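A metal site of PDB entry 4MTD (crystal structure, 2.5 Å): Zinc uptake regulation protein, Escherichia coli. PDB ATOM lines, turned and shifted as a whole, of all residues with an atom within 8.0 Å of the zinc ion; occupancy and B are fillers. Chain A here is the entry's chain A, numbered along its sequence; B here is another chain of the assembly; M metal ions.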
ATOM      1  N   ILE A 102      12.595  -3.796  12.639  1.00  0.00           N
ATOM      2  CA  ILE A 102      11.665  -2.714  12.949  1.00  0.00           C
ATOM      3  C   ILE A 102      11.678  -2.421  14.429  1.00  0.00           C
ATOM      4  O   ILE A 102      11.528  -3.325  15.252  1.00  0.00           O
ATOM      5  CB  ILE A 102      10.235  -3.108  12.552  1.00  0.00           C
ATOM      6  CG1 ILE A 102      10.187  -3.590  11.088  1.00  0.00           C
ATOM      7  CG2 ILE A 102       9.271  -1.947  12.766  1.00  0.00           C
ATOM      8  CD1 ILE A 102       9.173  -4.684  10.866  1.00  0.00           C
ATOM      9  N   CYS A 103      11.838  -1.155  14.783  1.00  0.00           N
ATOM     10  CA  CYS A 103      11.774  -0.754  16.165  1.00  0.00           C
ATOM     11  C   CYS A 103      10.333  -0.473  16.580  1.00  0.00           C
ATOM     12  O   CYS A 103       9.668   0.402  16.021  1.00  0.00           O
ATOM     13  CB  CYS A 103      12.639   0.470  16.392  1.00  0.00           C
ATOM     14  SG  CYS A 103      12.513   1.169  18.055  1.00  0.00           S
ATOM     15  N   ASP A 104       9.865  -1.219  17.579  1.00  0.00           N
ATOM     16  CA  ASP A 104       8.499  -1.120  18.082  1.00  0.00           C
ATOM     17  C   ASP A 104       8.256   0.143  18.901  1.00  0.00           C
ATOM     18  O   ASP A 104       7.110   0.462  19.214  1.00  0.00           O
ATOM     19  CB  ASP A 104       8.153  -2.337  18.953  1.00  0.00           C
ATOM     20  CG  ASP A 104       8.146  -3.637  18.171  1.00  0.00           C
ATOM     21  OD1 ASP A 104       7.772  -3.623  16.974  1.00  0.00           O
ATOM     22  OD2 ASP A 104       8.499  -4.674  18.770  1.00  0.00           O
ATOM     23  N   ARG A 105       9.320   0.839  19.270  1.00  0.00           N
ATOM     24  CA  ARG A 105       9.176   2.098  19.987  1.00  0.00           C
ATOM     25  C   ARG A 105       9.063   3.323  19.070  1.00  0.00           C
ATOM     26  O   ARG A 105       8.136   4.115  19.221  1.00  0.00           O
ATOM     27  CB  ARG A 105      10.316   2.268  20.985  1.00  0.00           C
ATOM     28  CG  ARG A 105      10.274   3.612  21.692  1.00  0.00           C
ATOM     29  CD  ARG A 105      11.068   3.622  22.983  1.00  0.00           C
ATOM     30  NE  ARG A 105      10.992   4.931  23.621  1.00  0.00           N
ATOM     31  CZ  ARG A 105      11.676   6.006  23.237  1.00  0.00           C
ATOM     32  NH1 ARG A 105      12.509   5.942  22.192  1.00  0.00           N
ATOM     33  NH2 ARG A 105      11.537   7.148  23.896  1.00  0.00           N
ATOM     34  N   CYS A 106      10.028   3.507  18.151  1.00  0.00           N
ATOM     35  CA  CYS A 106      10.124   4.731  17.331  1.00  0.00           C
ATOM     36  C   CYS A 106       9.734   4.578  15.837  1.00  0.00           C
ATOM     37  O   CYS A 106       9.682   5.569  15.114  1.00  0.00           O
ATOM     38  CB  CYS A 106      11.546   5.307  17.412  1.00  0.00           C
ATOM     39  SG  CYS A 106      12.770   4.385  16.456  1.00  0.00           S
ATOM     40  N   GLY A 107       9.495   3.356  15.385  1.00  0.00           N
ATOM     41  CA  GLY A 107       9.139   3.125  13.986  1.00  0.00           C
ATOM     42  C   GLY A 107      10.291   3.039  12.987  1.00  0.00           C
ATOM     43  O   GLY A 107      10.039   2.809  11.800  1.00  0.00           O
ATOM     44  N   ALA A 108      11.534   3.165  13.436  1.00  0.00           N
ATOM     45  CA  ALA A 108      12.678   3.112  12.508  1.00  0.00           C
ATOM     46  C   ALA A 108      12.840   1.709  11.974  1.00  0.00           C
ATOM     47  O   ALA A 108      12.411   0.749  12.602  1.00  0.00           O
ATOM     48  CB  ALA A 108      13.966   3.557  13.183  1.00  0.00           C
ATOM     49  N   VAL A 109      13.428   1.602  10.786  1.00  0.00           N
ATOM     50  CA  VAL A 109      13.563   0.331  10.094  1.00  0.00           C
ATOM     51  C   VAL A 109      14.919   0.261   9.390  1.00  0.00           C
ATOM     52  O   VAL A 109      15.229   1.101   8.561  1.00  0.00           O
ATOM     53  CB  VAL A 109      12.466   0.161   9.030  1.00  0.00           C
ATOM     54  CG1 VAL A 109      12.593  -1.198   8.332  1.00  0.00           C
ATOM     55  CG2 VAL A 109      11.085   0.302   9.658  1.00  0.00           C
ATOM     56  N   GLY A 141      11.632  -5.487  17.807  1.00  0.00           N
ATOM     57  CA  GLY A 141      12.596  -5.265  18.881  1.00  0.00           C
ATOM     58  C   GLY A 141      12.853  -3.787  19.030  1.00  0.00           C
ATOM     59  O   GLY A 141      11.960  -2.980  18.810  1.00  0.00           O
ATOM     60  N   LEU A 142      14.082  -3.428  19.386  1.00  0.00           N
ATOM     61  CA  LEU A 142      14.444  -2.031  19.578  1.00  0.00           C
ATOM     62  C   LEU A 142      15.743  -1.687  18.886  1.00  0.00           C
ATOM     63  O   LEU A 142      16.690  -2.464  18.906  1.00  0.00           O
ATOM     64  CB  LEU A 142      14.565  -1.693  21.062  1.00  0.00           C
ATOM     65  CG  LEU A 142      13.233  -1.792  21.814  1.00  0.00           C
ATOM     66  CD1 LEU A 142      13.034  -3.174  22.413  1.00  0.00           C
ATOM     67  CD2 LEU A 142      13.145  -0.719  22.888  1.00  0.00           C
ATOM     68  N   CYS A 143      15.769  -0.519  18.262  1.00  0.00           N
ATOM     69  CA  CYS A 143      16.969  -0.016  17.619  1.00  0.00           C
ATOM     70  C   CYS A 143      17.949   0.464  18.683  1.00  0.00           C
ATOM     71  O   CYS A 143      17.584   0.611  19.853  1.00  0.00           O
ATOM     72  CB  CYS A 143      16.614   1.097  16.631  1.00  0.00           C
ATOM     73  SG  CYS A 143      16.206   2.703  17.367  1.00  0.00           S
ATOM     74  N   ALA A 144      19.188   0.707  18.275  1.00  0.00           N
ATOM     75  CA  ALA A 144      20.253   1.102  19.190  1.00  0.00           C
ATOM     76  C   ALA A 144      19.831   2.259  20.098  1.00  0.00           C
ATOM     77  O   ALA A 144      19.833   2.127  21.325  1.00  0.00           O
ATOM     78  CB  ALA A 144      21.520   1.464  18.421  1.00  0.00           C
ATOM     79  N   ALA A 145      19.456   3.383  19.483  1.00  0.00           N
ATOM     80  CA  ALA A 145      19.058   4.592  20.219  1.00  0.00           C
ATOM     81  C   ALA A 145      18.007   4.303  21.272  1.00  0.00           C
ATOM     82  O   ALA A 145      18.114   4.768  22.406  1.00  0.00           O
ATOM     83  CB  ALA A 145      18.571   5.653  19.245  1.00  0.00           C
ATOM     84  N   CYS A 146      16.970   3.542  20.894  1.00  0.00           N
ATOM     85  CA  CYS A 146      15.874   3.232  21.827  1.00  0.00           C
ATOM     86  C   CYS A 146      16.305   2.231  22.882  1.00  0.00           C
ATOM     87  O   CYS A 146      15.689   2.156  23.957  1.00  0.00           O
ATOM     88  CB  CYS A 146      14.642   2.707  21.084  1.00  0.00           C
ATOM     89  SG  CYS A 146      13.807   3.904  20.016  1.00  0.00           S
ATOM     90  N   VAL A 147      17.332   1.434  22.598  1.00  0.00           N
ATOM     91  CA  VAL A 147      17.914   0.532  23.605  1.00  0.00           C
ATOM     92  C   VAL A 147      18.532   1.360  24.728  1.00  0.00           C
ATOM     93  O   VAL A 147      18.281   1.091  25.891  1.00  0.00           O
ATOM     94  CB  VAL A 147      18.953  -0.445  22.996  1.00  0.00           C
ATOM     95  CG1 VAL A 147      19.845  -1.054  24.082  1.00  0.00           C
ATOM     96  CG2 VAL A 147      18.256  -1.546  22.209  1.00  0.00           C
ATOM     97  N   VAL A 149      17.720   4.325  25.601  1.00  0.00           N
ATOM     98  CA  VAL A 149      16.642   5.040  26.280  1.00  0.00           C
ATOM     99  C   VAL A 149      15.865   4.151  27.243  1.00  0.00           C
ATOM    100  O   VAL A 149      15.431   4.618  28.303  1.00  0.00           O
ATOM    101  CB  VAL A 149      15.655   5.675  25.261  1.00  0.00           C
ATOM    102  CG1 VAL A 149      14.458   6.291  25.988  1.00  0.00           C
ATOM    103  CG2 VAL A 149      16.365   6.716  24.402  1.00  0.00           C
ATOM    104  N   PHE B 130      20.864  -3.562  17.741  1.00  0.00           N
ATOM    105  CA  PHE B 130      19.425  -3.848  17.709  1.00  0.00           C
ATOM    106  C   PHE B 130      19.076  -5.023  18.607  1.00  0.00           C
ATOM    107  O   PHE B 130      19.421  -6.156  18.308  1.00  0.00           O
ATOM    108  CB  PHE B 130      18.962  -4.105  16.262  1.00  0.00           C
ATOM    109  CG  PHE B 130      17.474  -4.234  16.096  1.00  0.00           C
ATOM    110  CD1 PHE B 130      16.714  -3.141  15.682  1.00  0.00           C
ATOM    111  CD2 PHE B 130      16.833  -5.440  16.295  1.00  0.00           C
ATOM    112  CE1 PHE B 130      15.344  -3.243  15.499  1.00  0.00           C
ATOM    113  CE2 PHE B 130      15.463  -5.563  16.126  1.00  0.00           C
ATOM    114  CZ  PHE B 130      14.718  -4.464  15.728  1.00  0.00           C
HETATM  115 ZN    ZN M   1      13.954   2.971  17.906  1.00  0.00          ZN
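SG of Cys 146 binds the zinc ion (2.3 Å). The zinc ion is bound by the side-chain sulfur (SG) of Cys 103, at 2.3 Å. The side-chain sulfur (SG) of Cys 143 is bound to the zinc ion (2.3 Å). The zinc ion is bound by SG of Cys 106 (2.3 Å).
SG of Cys 146 sits close to NH1 of Arg 105. O of Ala 108 lies within hydrogen-bond range of N of Cys 103, at 3.0 Å. The backbone NH of Arg 105 lies close to the side-chain sulfur of Cys 103 (3.4 Å). N of Ala 108 lies close to SG of Cys 106 (3.5 Å).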
